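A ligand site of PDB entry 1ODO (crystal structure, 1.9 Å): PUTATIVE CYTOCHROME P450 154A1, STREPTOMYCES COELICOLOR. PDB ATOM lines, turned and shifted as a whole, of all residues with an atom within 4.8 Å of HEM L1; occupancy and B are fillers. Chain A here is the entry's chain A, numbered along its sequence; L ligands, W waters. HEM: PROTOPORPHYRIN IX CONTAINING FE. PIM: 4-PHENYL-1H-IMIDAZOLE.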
ATOM      1  N   LEU A  53      24.954  -4.799 -11.418  1.00  0.00           N
ATOM      2  CA  LEU A  53      24.818  -3.416 -10.977  1.00  0.00           C
ATOM      3  C   LEU A  53      24.051  -2.493 -11.934  1.00  0.00           C
ATOM      4  O   LEU A  53      23.813  -1.318 -11.618  1.00  0.00           O
ATOM      5  CB  LEU A  53      26.206  -2.821 -10.720  1.00  0.00           C
ATOM      6  CG  LEU A  53      27.010  -3.458  -9.579  1.00  0.00           C
ATOM      7  CD1 LEU A  53      28.430  -2.882  -9.519  1.00  0.00           C
ATOM      8  CD2 LEU A  53      26.290  -3.215  -8.268  1.00  0.00           C
ATOM      9  N   LYS A  60      18.638  -2.695  -4.129  1.00  0.00           N
ATOM     10  CA  LYS A  60      19.252  -2.361  -2.851  1.00  0.00           C
ATOM     11  C   LYS A  60      18.142  -2.107  -1.825  1.00  0.00           C
ATOM     12  O   LYS A  60      18.412  -1.783  -0.672  1.00  0.00           O
ATOM     13  CB  LYS A  60      20.121  -1.096  -2.954  1.00  0.00           C
ATOM     14  CG  LYS A  60      21.337  -1.213  -3.869  1.00  0.00           C
ATOM     15  CD  LYS A  60      22.409  -0.214  -3.458  1.00  0.00           C
ATOM     16  CE  LYS A  60      23.041  -0.602  -2.120  1.00  0.00           C
ATOM     17  NZ  LYS A  60      23.797   0.506  -1.484  1.00  0.00           N
ATOM     18  N   MET A  87      18.913   7.122  -0.400  1.00  0.00           N
ATOM     19  CA  MET A  87      19.255   6.647  -1.739  1.00  0.00           C
ATOM     20  C   MET A  87      20.049   5.338  -1.729  1.00  0.00           C
ATOM     21  O   MET A  87      19.957   4.549  -2.677  1.00  0.00           O
ATOM     22  CB  MET A  87      20.050   7.712  -2.492  1.00  0.00           C
ATOM     23  CG  MET A  87      21.486   7.882  -2.018  1.00  0.00           C
ATOM     24  SD  MET A  87      22.357   9.174  -2.936  1.00  0.00           S
ATOM     25  CE  MET A  87      21.948  10.615  -1.934  1.00  0.00           C
ATOM     26  N   PHE A  88      20.802   5.109  -0.661  1.00  0.00           N
ATOM     27  CA  PHE A  88      21.621   3.904  -0.511  1.00  0.00           C
ATOM     28  C   PHE A  88      20.800   2.612  -0.464  1.00  0.00           C
ATOM     29  O   PHE A  88      21.317   1.523  -0.717  1.00  0.00           O
ATOM     30  CB  PHE A  88      22.473   4.027   0.775  1.00  0.00           C
ATOM     31  CG  PHE A  88      23.600   3.026   0.865  1.00  0.00           C
ATOM     32  CD1 PHE A  88      24.754   3.192   0.106  1.00  0.00           C
ATOM     33  CD2 PHE A  88      23.520   1.941   1.730  1.00  0.00           C
ATOM     34  CE1 PHE A  88      25.818   2.290   0.208  1.00  0.00           C
ATOM     35  CE2 PHE A  88      24.572   1.037   1.850  1.00  0.00           C
ATOM     36  CZ  PHE A  88      25.717   1.207   1.081  1.00  0.00           C
ATOM     37  N   HIS A  95      14.944   5.773  -6.144  1.00  0.00           N
ATOM     38  CA  HIS A  95      16.368   6.018  -5.984  1.00  0.00           C
ATOM     39  C   HIS A  95      16.744   7.294  -6.739  1.00  0.00           C
ATOM     40  O   HIS A  95      17.488   8.127  -6.219  1.00  0.00           O
ATOM     41  CB  HIS A  95      17.197   4.856  -6.527  1.00  0.00           C
ATOM     42  CG  HIS A  95      18.646   5.186  -6.677  1.00  0.00           C
ATOM     43  ND1 HIS A  95      19.243   5.421  -7.897  1.00  0.00           N
ATOM     44  CD2 HIS A  95      19.617   5.396  -5.743  1.00  0.00           C
ATOM     45  CE1 HIS A  95      20.505   5.771  -7.722  1.00  0.00           C
ATOM     46  NE2 HIS A  95      20.755   5.756  -6.416  1.00  0.00           N
ATOM     47  N   ARG A  99      18.407  10.514  -4.817  1.00  0.00           N
ATOM     48  CA  ARG A  99      19.783  10.860  -5.173  1.00  0.00           C
ATOM     49  C   ARG A  99      19.823  12.263  -5.766  1.00  0.00           C
ATOM     50  O   ARG A  99      20.714  13.056  -5.446  1.00  0.00           O
ATOM     51  CB  ARG A  99      20.362   9.856  -6.190  1.00  0.00           C
ATOM     52  CG  ARG A  99      21.801  10.159  -6.648  1.00  0.00           C
ATOM     53  CD  ARG A  99      22.264   9.114  -7.677  1.00  0.00           C
ATOM     54  NE  ARG A  99      23.540   9.428  -8.313  1.00  0.00           N
ATOM     55  CZ  ARG A  99      24.709   8.887  -7.976  1.00  0.00           C
ATOM     56  NH1 ARG A  99      24.794   7.995  -6.994  1.00  0.00           N
ATOM     57  NH2 ARG A  99      25.805   9.222  -8.653  1.00  0.00           N
ATOM     58  N   PHE A 106      27.322  17.886  -5.627  1.00  0.00           N
ATOM     59  CA  PHE A 106      28.486  17.145  -6.104  1.00  0.00           C
ATOM     60  C   PHE A 106      28.666  17.189  -7.612  1.00  0.00           C
ATOM     61  O   PHE A 106      29.354  16.341  -8.188  1.00  0.00           O
ATOM     62  CB  PHE A 106      28.428  15.698  -5.626  1.00  0.00           C
ATOM     63  CG  PHE A 106      28.377  15.565  -4.139  1.00  0.00           C
ATOM     64  CD1 PHE A 106      27.181  15.720  -3.447  1.00  0.00           C
ATOM     65  CD2 PHE A 106      29.537  15.323  -3.411  1.00  0.00           C
ATOM     66  CE1 PHE A 106      27.138  15.631  -2.060  1.00  0.00           C
ATOM     67  CE2 PHE A 106      29.506  15.241  -2.021  1.00  0.00           C
ATOM     68  CZ  PHE A 106      28.312  15.390  -1.351  1.00  0.00           C
ATOM     69  N   ILE A 153      33.682  17.814   4.428  1.00  0.00           N
ATOM     70  CA  ILE A 153      32.269  17.486   4.597  1.00  0.00           C
ATOM     71  C   ILE A 153      31.600  18.470   5.554  1.00  0.00           C
ATOM     72  O   ILE A 153      30.418  18.787   5.390  1.00  0.00           O
ATOM     73  CB  ILE A 153      32.091  16.034   5.117  1.00  0.00           C
ATOM     74  CG1 ILE A 153      30.650  15.578   4.870  1.00  0.00           C
ATOM     75  CG2 ILE A 153      32.418  15.951   6.608  1.00  0.00           C
ATOM     76  CD1 ILE A 153      30.287  15.499   3.408  1.00  0.00           C
ATOM     77  N   LEU A 238      24.017   9.119   6.036  1.00  0.00           N
ATOM     78  CA  LEU A 238      24.794   8.666   4.896  1.00  0.00           C
ATOM     79  C   LEU A 238      25.865   9.674   4.478  1.00  0.00           C
ATOM     80  O   LEU A 238      27.032   9.325   4.326  1.00  0.00           O
ATOM     81  CB  LEU A 238      23.871   8.412   3.698  1.00  0.00           C
ATOM     82  CG  LEU A 238      24.521   8.198   2.329  1.00  0.00           C
ATOM     83  CD1 LEU A 238      25.396   6.947   2.346  1.00  0.00           C
ATOM     84  CD2 LEU A 238      23.427   8.048   1.271  1.00  0.00           C
ATOM     85  N   MET A 239      25.460  10.927   4.292  1.00  0.00           N
ATOM     86  CA  MET A 239      26.398  11.964   3.893  1.00  0.00           C
ATOM     87  C   MET A 239      27.493  12.241   4.907  1.00  0.00           C
ATOM     88  O   MET A 239      28.650  12.414   4.555  1.00  0.00           O
ATOM     89  CB  MET A 239      25.648  13.246   3.562  1.00  0.00           C
ATOM     90  CG  MET A 239      24.548  13.061   2.514  1.00  0.00           C
ATOM     91  SD  MET A 239      25.129  12.242   1.010  1.00  0.00           S
ATOM     92  CE  MET A 239      26.348  13.416   0.489  1.00  0.00           C
ATOM     93  N   ALA A 242      29.829   9.129   5.107  1.00  0.00           N
ATOM     94  CA  ALA A 242      30.654   9.049   3.918  1.00  0.00           C
ATOM     95  C   ALA A 242      31.798  10.056   3.954  1.00  0.00           C
ATOM     96  O   ALA A 242      32.901   9.783   3.462  1.00  0.00           O
ATOM     97  CB  ALA A 242      29.801   9.267   2.682  1.00  0.00           C
ATOM     98  N   GLY A 243      31.553  11.224   4.532  1.00  0.00           N
ATOM     99  CA  GLY A 243      32.593  12.232   4.600  1.00  0.00           C
ATOM    100  C   GLY A 243      33.595  12.040   5.735  1.00  0.00           C
ATOM    101  O   GLY A 243      34.728  12.486   5.636  1.00  0.00           O
ATOM    102  N   THR A 246      36.129   6.386   5.002  1.00  0.00           N
ATOM    103  CA  THR A 246      36.391   6.051   3.612  1.00  0.00           C
ATOM    104  C   THR A 246      37.462   6.905   2.911  1.00  0.00           C
ATOM    105  O   THR A 246      38.508   6.373   2.557  1.00  0.00           O
ATOM    106  CB  THR A 246      35.095   6.086   2.786  1.00  0.00           C
ATOM    107  OG1 THR A 246      33.988   5.787   3.643  1.00  0.00           O
ATOM    108  CG2 THR A 246      35.147   5.027   1.700  1.00  0.00           C
ATOM    109  N   THR A 247      37.228   8.203   2.688  1.00  0.00           N
ATOM    110  CA  THR A 247      38.284   8.967   2.030  1.00  0.00           C
ATOM    111  C   THR A 247      39.602   8.861   2.812  1.00  0.00           C
ATOM    112  O   THR A 247      40.688   8.854   2.223  1.00  0.00           O
ATOM    113  CB  THR A 247      37.914  10.459   1.836  1.00  0.00           C
ATOM    114  OG1 THR A 247      36.733  10.548   1.028  1.00  0.00           O
ATOM    115  CG2 THR A 247      39.043  11.199   1.123  1.00  0.00           C
ATOM    116  N   VAL A 250      41.732   6.152   1.517  1.00  0.00           N
ATOM    117  CA  VAL A 250      42.335   6.331   0.215  1.00  0.00           C
ATOM    118  C   VAL A 250      43.614   7.130   0.412  1.00  0.00           C
ATOM    119  O   VAL A 250      44.648   6.842  -0.200  1.00  0.00           O
ATOM    120  CB  VAL A 250      41.403   7.094  -0.743  1.00  0.00           C
ATOM    121  CG1 VAL A 250      42.032   7.156  -2.128  1.00  0.00           C
ATOM    122  CG2 VAL A 250      40.045   6.396  -0.813  1.00  0.00           C
ATOM    123  N   LEU A 283      42.960   3.417  -5.943  1.00  0.00           N
ATOM    124  CA  LEU A 283      41.553   3.040  -5.872  1.00  0.00           C
ATOM    125  C   LEU A 283      41.363   1.618  -6.405  1.00  0.00           C
ATOM    126  O   LEU A 283      40.504   0.867  -5.936  1.00  0.00           O
ATOM    127  CB  LEU A 283      40.701   4.021  -6.677  1.00  0.00           C
ATOM    128  CG  LEU A 283      40.584   5.406  -6.027  1.00  0.00           C
ATOM    129  CD1 LEU A 283      39.935   6.408  -6.968  1.00  0.00           C
ATOM    130  CD2 LEU A 283      39.767   5.257  -4.756  1.00  0.00           C
ATOM    131  N   ALA A 288      39.090   1.731  -0.640  1.00  0.00           N
ATOM    132  CA  ALA A 288      38.649   1.932   0.742  1.00  0.00           C
ATOM    133  C   ALA A 288      37.504   1.051   1.210  1.00  0.00           C
ATOM    134  O   ALA A 288      37.389   0.762   2.407  1.00  0.00           O
ATOM    135  CB  ALA A 288      38.293   3.413   0.960  1.00  0.00           C
ATOM    136  N   VAL A 289      36.636   0.628   0.283  1.00  0.00           N
ATOM    137  CA  VAL A 289      35.510  -0.225   0.619  1.00  0.00           C
ATOM    138  C   VAL A 289      35.704  -1.566  -0.100  1.00  0.00           C
ATOM    139  O   VAL A 289      35.596  -1.638  -1.324  1.00  0.00           O
ATOM    140  CB  VAL A 289      34.185   0.424   0.171  1.00  0.00           C
ATOM    141  CG1 VAL A 289      33.009  -0.524   0.433  1.00  0.00           C
ATOM    142  CG2 VAL A 289      33.988   1.727   0.923  1.00  0.00           C
ATOM    143  N   LEU A 292      30.445  -4.431  -0.418  1.00  0.00           N
ATOM    144  CA  LEU A 292      29.316  -3.530  -0.249  1.00  0.00           C
ATOM    145  C   LEU A 292      27.987  -4.206   0.057  1.00  0.00           C
ATOM    146  O   LEU A 292      27.357  -4.783  -0.830  1.00  0.00           O
ATOM    147  CB  LEU A 292      29.170  -2.643  -1.492  1.00  0.00           C
ATOM    148  CG  LEU A 292      28.386  -1.322  -1.440  1.00  0.00           C
ATOM    149  CD1 LEU A 292      26.894  -1.584  -1.223  1.00  0.00           C
ATOM    150  CD2 LEU A 292      28.950  -0.451  -0.316  1.00  0.00           C
ATOM    151  N   ARG A 295      22.699  -6.239  -1.782  1.00  0.00           N
ATOM    152  CA  ARG A 295      21.736  -6.167  -2.881  1.00  0.00           C
ATOM    153  C   ARG A 295      20.921  -7.459  -2.884  1.00  0.00           C
ATOM    154  O   ARG A 295      21.315  -8.433  -2.260  1.00  0.00           O
ATOM    155  CB  ARG A 295      22.455  -5.983  -4.212  1.00  0.00           C
ATOM    156  CG  ARG A 295      22.850  -4.527  -4.478  1.00  0.00           C
ATOM    157  CD  ARG A 295      23.572  -4.388  -5.810  1.00  0.00           C
ATOM    158  NE  ARG A 295      23.702  -2.994  -6.242  1.00  0.00           N
ATOM    159  CZ  ARG A 295      24.579  -2.132  -5.747  1.00  0.00           C
ATOM    160  NH1 ARG A 295      25.437  -2.480  -4.795  1.00  0.00           N
ATOM    161  NH2 ARG A 295      24.605  -0.886  -6.213  1.00  0.00           N
ATOM    162  N   TYR A 319      34.157  -5.561  -4.390  1.00  0.00           N
ATOM    163  CA  TYR A 319      34.976  -4.662  -5.197  1.00  0.00           C
ATOM    164  C   TYR A 319      36.485  -4.807  -5.158  1.00  0.00           C
ATOM    165  O   TYR A 319      37.144  -4.771  -6.215  1.00  0.00           O
ATOM    166  CB  TYR A 319      34.597  -3.222  -4.840  1.00  0.00           C
ATOM    167  CG  TYR A 319      33.167  -2.885  -5.197  1.00  0.00           C
ATOM    168  CD1 TYR A 319      32.401  -2.081  -4.358  1.00  0.00           C
ATOM    169  CD2 TYR A 319      32.599  -3.332  -6.386  1.00  0.00           C
ATOM    170  CE1 TYR A 319      31.091  -1.730  -4.690  1.00  0.00           C
ATOM    171  CE2 TYR A 319      31.294  -2.983  -6.733  1.00  0.00           C
ATOM    172  CZ  TYR A 319      30.544  -2.180  -5.887  1.00  0.00           C
ATOM    173  OH  TYR A 319      29.267  -1.825  -6.224  1.00  0.00           O
ATOM    174  N   ALA A 346      36.070   0.756  -7.335  1.00  0.00           N
ATOM    175  CA  ALA A 346      36.136   1.312  -5.985  1.00  0.00           C
ATOM    176  C   ALA A 346      34.907   2.164  -5.649  1.00  0.00           C
ATOM    177  O   ALA A 346      34.477   2.223  -4.487  1.00  0.00           O
ATOM    178  CB  ALA A 346      37.401   2.151  -5.828  1.00  0.00           C
ATOM    179  N   PHE A 347      34.327   2.806  -6.659  1.00  0.00           N
ATOM    180  CA  PHE A 347      33.148   3.648  -6.485  1.00  0.00           C
ATOM    181  C   PHE A 347      31.857   2.993  -6.959  1.00  0.00           C
ATOM    182  O   PHE A 347      30.802   3.634  -6.974  1.00  0.00           O
ATOM    183  CB  PHE A 347      33.313   4.963  -7.242  1.00  0.00           C
ATOM    184  CG  PHE A 347      34.388   5.861  -6.705  1.00  0.00           C
ATOM    185  CD1 PHE A 347      35.419   6.314  -7.539  1.00  0.00           C
ATOM    186  CD2 PHE A 347      34.355   6.297  -5.383  1.00  0.00           C
ATOM    187  CE1 PHE A 347      36.381   7.195  -7.054  1.00  0.00           C
ATOM    188  CE2 PHE A 347      35.318   7.178  -4.898  1.00  0.00           C
ATOM    189  CZ  PHE A 347      36.329   7.628  -5.746  1.00  0.00           C
ATOM    190  N   GLY A 348      31.930   1.731  -7.352  1.00  0.00           N
ATOM    191  CA  GLY A 348      30.733   1.071  -7.815  1.00  0.00           C
ATOM    192  C   GLY A 348      30.577   1.242  -9.317  1.00  0.00           C
ATOM    193  O   GLY A 348      31.527   1.562 -10.021  1.00  0.00           O
ATOM    194  N   VAL A 351      23.804   3.480 -11.589  1.00  0.00           N
ATOM    195  CA  VAL A 351      23.068   4.543 -10.912  1.00  0.00           C
ATOM    196  C   VAL A 351      23.485   4.872  -9.497  1.00  0.00           C
ATOM    197  O   VAL A 351      23.311   6.006  -9.041  1.00  0.00           O
ATOM    198  CB  VAL A 351      21.547   4.273 -10.944  1.00  0.00           C
ATOM    199  CG1 VAL A 351      21.065   4.197 -12.380  1.00  0.00           C
ATOM    200  CG2 VAL A 351      21.217   2.983 -10.202  1.00  0.00           C
ATOM    201  N   HIS A 352      24.042   3.891  -8.794  1.00  0.00           N
ATOM    202  CA  HIS A 352      24.484   4.095  -7.409  1.00  0.00           C
ATOM    203  C   HIS A 352      25.948   4.529  -7.317  1.00  0.00           C
ATOM    204  O   HIS A 352      26.465   4.724  -6.214  1.00  0.00           O
ATOM    205  CB  HIS A 352      24.279   2.809  -6.602  1.00  0.00           C
ATOM    206  CG  HIS A 352      22.843   2.439  -6.376  1.00  0.00           C
ATOM    207  ND1 HIS A 352      22.093   2.967  -5.348  1.00  0.00           N
ATOM    208  CD2 HIS A 352      22.022   1.610  -7.058  1.00  0.00           C
ATOM    209  CE1 HIS A 352      20.866   2.462  -5.396  1.00  0.00           C
ATOM    210  NE2 HIS A 352      20.799   1.640  -6.422  1.00  0.00           N
ATOM    211  N   PHE A 353      26.603   4.665  -8.462  1.00  0.00           N
ATOM    212  CA  PHE A 353      28.010   5.078  -8.492  1.00  0.00           C
ATOM    213  C   PHE A 353      28.227   6.174  -7.446  1.00  0.00           C
ATOM    214  O   PHE A 353      27.502   7.165  -7.426  1.00  0.00           O
ATOM    215  CB  PHE A 353      28.373   5.618  -9.881  1.00  0.00           C
ATOM    216  CG  PHE A 353      29.849   5.854 -10.078  1.00  0.00           C
ATOM    217  CD1 PHE A 353      30.663   4.857 -10.593  1.00  0.00           C
ATOM    218  CD2 PHE A 353      30.413   7.081  -9.725  1.00  0.00           C
ATOM    219  CE1 PHE A 353      32.041   5.066 -10.745  1.00  0.00           C
ATOM    220  CE2 PHE A 353      31.787   7.299  -9.879  1.00  0.00           C
ATOM    221  CZ  PHE A 353      32.597   6.290 -10.387  1.00  0.00           C
ATOM    222  N   CYS A 354      29.229   5.980  -6.590  1.00  0.00           N
ATOM    223  CA  CYS A 354      29.531   6.948  -5.537  1.00  0.00           C
ATOM    224  C   CYS A 354      29.292   8.407  -5.916  1.00  0.00           C
ATOM    225  O   CYS A 354      29.954   8.954  -6.797  1.00  0.00           O
ATOM    226  CB  CYS A 354      30.975   6.804  -5.069  1.00  0.00           C
ATOM    227  SG  CYS A 354      31.332   7.937  -3.716  1.00  0.00           S
ATOM    228  N   LEU A 355      28.349   9.044  -5.238  1.00  0.00           N
ATOM    229  CA  LEU A 355      28.011  10.441  -5.493  1.00  0.00           C
ATOM    230  C   LEU A 355      29.179  11.360  -5.130  1.00  0.00           C
ATOM    231  O   LEU A 355      29.374  12.402  -5.755  1.00  0.00           O
ATOM    232  CB  LEU A 355      26.765  10.823  -4.694  1.00  0.00           C
ATOM    233  CG  LEU A 355      26.109  12.164  -5.000  1.00  0.00           C
ATOM    234  CD1 LEU A 355      25.614  12.183  -6.443  1.00  0.00           C
ATOM    235  CD2 LEU A 355      24.950  12.386  -4.032  1.00  0.00           C
ATOM    236  N   GLY A 356      29.960  10.975  -4.125  1.00  0.00           N
ATOM    237  CA  GLY A 356      31.087  11.795  -3.704  1.00  0.00           C
ATOM    238  C   GLY A 356      32.399  11.570  -4.446  1.00  0.00           C
ATOM    239  O   GLY A 356      33.398  12.227  -4.148  1.00  0.00           O
ATOM    240  N   LEU A 359      34.594  14.594  -5.500  1.00  0.00           N
ATOM    241  CA  LEU A 359      35.117  15.324  -4.344  1.00  0.00           C
ATOM    242  C   LEU A 359      36.229  14.510  -3.679  1.00  0.00           C
ATOM    243  O   LEU A 359      37.277  15.059  -3.322  1.00  0.00           O
ATOM    244  CB  LEU A 359      33.994  15.611  -3.341  1.00  0.00           C
ATOM    245  CG  LEU A 359      34.386  16.435  -2.106  1.00  0.00           C
ATOM    246  CD1 LEU A 359      35.033  17.739  -2.545  1.00  0.00           C
ATOM    247  CD2 LEU A 359      33.154  16.702  -1.251  1.00  0.00           C
ATOM    248  N   ALA A 360      36.014  13.217  -3.506  1.00  0.00           N
ATOM    249  CA  ALA A 360      37.019  12.357  -2.881  1.00  0.00           C
ATOM    250  C   ALA A 360      38.295  12.376  -3.723  1.00  0.00           C
ATOM    251  O   ALA A 360      39.400  12.523  -3.202  1.00  0.00           O
ATOM    252  CB  ALA A 360      36.503  10.930  -2.735  1.00  0.00           C
ATOM    253  N   GLU A 363      40.086  15.612  -3.150  1.00  0.00           N
ATOM    254  CA  GLU A 363      40.679  15.648  -1.814  1.00  0.00           C
ATOM    255  C   GLU A 363      42.013  14.910  -1.760  1.00  0.00           C
ATOM    256  O   GLU A 363      43.009  15.438  -1.260  1.00  0.00           O
ATOM    257  CB  GLU A 363      39.734  15.033  -0.775  1.00  0.00           C
ATOM    258  CG  GLU A 363      38.563  15.919  -0.385  1.00  0.00           C
ATOM    259  CD  GLU A 363      37.718  15.306   0.720  1.00  0.00           C
ATOM    260  OE1 GLU A 363      38.299  14.742   1.676  1.00  0.00           O
ATOM    261  OE2 GLU A 363      36.475  15.394   0.643  1.00  0.00           O
HETATM  262  CHA HEM L   1      28.067   5.197  -2.469  1.00  0.00           C
HETATM  263  CHB HEM L   1      28.880   9.690  -0.926  1.00  0.00           C
HETATM  264  CHC HEM L   1      33.617   8.786  -0.757  1.00  0.00           C
HETATM  265  CHD HEM L   1      32.782   4.302  -2.271  1.00  0.00           C
HETATM  266  C1A HEM L   1      27.852   6.499  -2.084  1.00  0.00           C
HETATM  267  C2A HEM L   1      26.555   7.169  -1.998  1.00  0.00           C
HETATM  268  C3A HEM L   1      26.776   8.422  -1.570  1.00  0.00           C
HETATM  269  C4A HEM L   1      28.209   8.580  -1.366  1.00  0.00           C
HETATM  270  CMA HEM L   1      25.733   9.528  -1.304  1.00  0.00           C
HETATM  271  CAA HEM L   1      25.203   6.505  -2.356  1.00  0.00           C
HETATM  272  CBA HEM L   1      24.948   6.583  -3.874  1.00  0.00           C
HETATM  273  CGA HEM L   1      23.638   5.942  -4.348  1.00  0.00           C
HETATM  274  O1A HEM L   1      23.276   4.894  -3.720  1.00  0.00           O
HETATM  275  O2A HEM L   1      23.044   6.469  -5.290  1.00  0.00           O
HETATM  276  C1B HEM L   1      30.219   9.840  -0.738  1.00  0.00           C
HETATM  277  C2B HEM L   1      30.854  11.061  -0.255  1.00  0.00           C
HETATM  278  C3B HEM L   1      32.190  10.805  -0.202  1.00  0.00           C
HETATM  279  C4B HEM L   1      32.398   9.446  -0.651  1.00  0.00           C
HETATM  280  CMB HEM L   1      30.096  12.350   0.118  1.00  0.00           C
HETATM  281  CAB HEM L   1      33.334  11.744   0.233  1.00  0.00           C
HETATM  282  CBB HEM L   1      33.541  12.970  -0.665  1.00  0.00           C
HETATM  283  C1C HEM L   1      33.796   7.470  -1.168  1.00  0.00           C
HETATM  284  C2C HEM L   1      35.116   6.814  -1.247  1.00  0.00           C
HETATM  285  C3C HEM L   1      34.879   5.555  -1.665  1.00  0.00           C
HETATM  286  C4C HEM L   1      33.448   5.428  -1.849  1.00  0.00           C
HETATM  287  CMC HEM L   1      36.457   7.521  -0.883  1.00  0.00           C
HETATM  288  CAC HEM L   1      35.853   4.366  -1.930  1.00  0.00           C
HETATM  289  CBC HEM L   1      37.114   4.676  -2.750  1.00  0.00           C
HETATM  290  C1D HEM L   1      31.438   4.141  -2.451  1.00  0.00           C
HETATM  291  C2D HEM L   1      30.790   2.917  -2.879  1.00  0.00           C
HETATM  292  C3D HEM L   1      29.462   3.169  -2.921  1.00  0.00           C
HETATM  293  C4D HEM L   1      29.280   4.545  -2.541  1.00  0.00           C
HETATM  294  CMD HEM L   1      31.524   1.598  -3.189  1.00  0.00           C
HETATM  295  CAD HEM L   1      28.366   2.148  -3.285  1.00  0.00           C
HETATM  296  CBD HEM L   1      28.265   1.682  -4.740  1.00  0.00           C
HETATM  297  CGD HEM L   1      27.165   0.656  -4.797  1.00  0.00           C
HETATM  298  O1D HEM L   1      27.461  -0.532  -4.986  1.00  0.00           O
HETATM  299  O2D HEM L   1      25.995   1.074  -4.607  1.00  0.00           O
HETATM  300  NA  HEM L   1      28.833   7.381  -1.705  1.00  0.00           N
HETATM  301  NB  HEM L   1      31.191   8.873  -0.962  1.00  0.00           N
HETATM  302  NC  HEM L   1      32.809   6.609  -1.543  1.00  0.00           N
HETATM  303  ND  HEM L   1      30.498   5.145  -2.236  1.00  0.00           N
HETATM  304 FE   HEM L   1      30.832   6.994  -1.628  1.00  0.00          FE
HETATM  305  N1  PIM L   2      30.871   5.792   2.594  1.00  0.00           N
HETATM  306  C2  PIM L   2      31.466   6.292   1.439  1.00  0.00           C
HETATM  307  N3  PIM L   2      30.620   6.309   0.537  1.00  0.00           N
HETATM  308  C4  PIM L   2      29.466   5.839   0.985  1.00  0.00           C
HETATM  309  C5  PIM L   2      29.593   5.505   2.270  1.00  0.00           C
HETATM  310  C6  PIM L   2      28.605   4.944   3.252  1.00  0.00           C
HETATM  311  C7  PIM L   2      28.780   5.232   4.648  1.00  0.00           C
HETATM  312  C8  PIM L   2      27.833   4.691   5.588  1.00  0.00           C
HETATM  313  C9  PIM L   2      26.767   3.896   5.103  1.00  0.00           C
HETATM  314  C10 PIM L   2      26.600   3.604   3.718  1.00  0.00           C
HETATM  315  C11 PIM L   2      27.558   4.150   2.818  1.00  0.00           C
HETATM  316  O   HOH W   1      35.142  11.129   3.145  1.00  0.00           O
HETATM  317  O   HOH W   2      27.448   0.694  -7.765  1.00  0.00           O
HETATM  318  O   HOH W   3      24.745   2.656  -2.964  1.00  0.00           O
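The guanidinium group (NH1) of Arg 99 is in salt-bridge range of an oxygen (O2A) of HEM L1 (2.9 Å).
An iron atom (FE) of HEM L1 is bound by the side-chain sulfur of Cys 354, 2.3 Å away.
The side-chain amino group (NZ) of Lys 60 is in salt-bridge range of an oxygen (O2D) of HEM L1 (3.9 Å).
OG1 of Thr 246 lies within hydrogen-bond range of N1 of PIM L2.
The guanidinium group of Arg 295 lies within salt-bridge range of an oxygen (O1D) of HEM L1, at 2.8 Å.
OH of Tyr 319 is in hydrogen-bond range of O1D of HEM L1.
An oxygen (O2A) of HEM L1 lies within hydrogen-bond range of a ring nitrogen (NE2) of His 95 (2.6 Å).
An oxygen (O1A) of HEM L1 sits at hydrogen-bond distance from a ring nitrogen (ND1) of His 352, 2.8 Å away.
FE of HEM L1 is bound by N3 of PIM L2, at 2.3 Å.
The side-chain sulfur (SG) of Cys 354 sits close to the backbone NH (N) of Gly 356 (3.4 Å).
NE2 of His 95 lies within hydrogen-bond range of ND1 of His 352.
The guanidinium group (NH1) of Arg 99 is in hydrogen-bond range of the backbone carbonyl oxygen (O) of Val 351 (3.2 Å).
The backbone carbonyl oxygen (O) of Phe 88 lies within hydrogen-bond range of the side-chain amino group (NZ) of Lys 60, at 2.8 Å.
The backbone NH of Cys 354 is in hydrogen-bond range of the backbone carbonyl oxygen of Phe 347, 2.9 Å away.
NH1 of Arg 99 is in hydrogen-bond range of O of Phe 353 (2.9 Å).
The backbone carbonyl oxygen of Met 87 sits close to an oxygen (O1A) of HEM L1.
CA of Phe 88 touches O1A of HEM L1, at 3.7 Å.
Phe 106 touches HEM L1 (CE2 to CMB, 3.6 Å).
Leu 238 touches HEM L1.
Met 239 touches HEM L1 (SD to CMA, 3.6 Å).
Ala 242 touches HEM L1.
Thr 246 touches HEM L1.
Thr 247 touches HEM L1 (OG1 to CMC, 3.6 Å).
CG2 of Val 250 touches CMC of HEM L1, 3.8 Å away.
Leu 283 touches HEM L1 (CD2 to CBC, 3.4 Å).
Ala 288 touches HEM L1 (CB to CAC, 3.9 Å).
Leu 292 touches HEM L1.
Ala 346 touches HEM L1 (O to CMD, 3.3 Å).
Phe 347 touches HEM L1 (CE2 to C3C, 3.6 Å).
Gly 348 touches HEM L1 (CA to CBD, 3.99 Å).
Val 351 touches HEM L1 (O to O2A, 3.8 Å).
Leu 355 touches HEM L1.
Gly 356 touches HEM L1 (CA to C2B, 3.5 Å).
CB of Leu 359 touches CBB of HEM L1 (3.8 Å).
Ala 360 touches HEM L1 (N to CBB, 3.8 Å).
Within 4 Å of HEM L1: Lys 60, Met 87, Phe 88, His 95, Arg 99, Phe 106, Leu 238, Met 239, Ala 242, Thr 246, Thr 247, Val 250, Leu 283, Ala 288, Leu 292, Arg 295, Tyr 319, Ala 346, Phe 347, Gly 348, Val 351, His 352, Cys 354, Leu 355, Gly 356, Leu 359 and Ala 360.
Water W3 bridges an oxygen (O2D) of HEM L1 (2.6 Å) and the side-chain amino group of Lys 60 (2.8 Å).
Water W2 lies within hydrogen-bond range of an oxygen (O1D) of HEM L1 and the side-chain hydroxyl (OH) of Tyr 319.
Water W1 lies within hydrogen-bond range of O of Ala 242 (2.6 Å), OG1 of Thr 247 (2.7 Å) and O of Gly 243 (2.9 Å).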
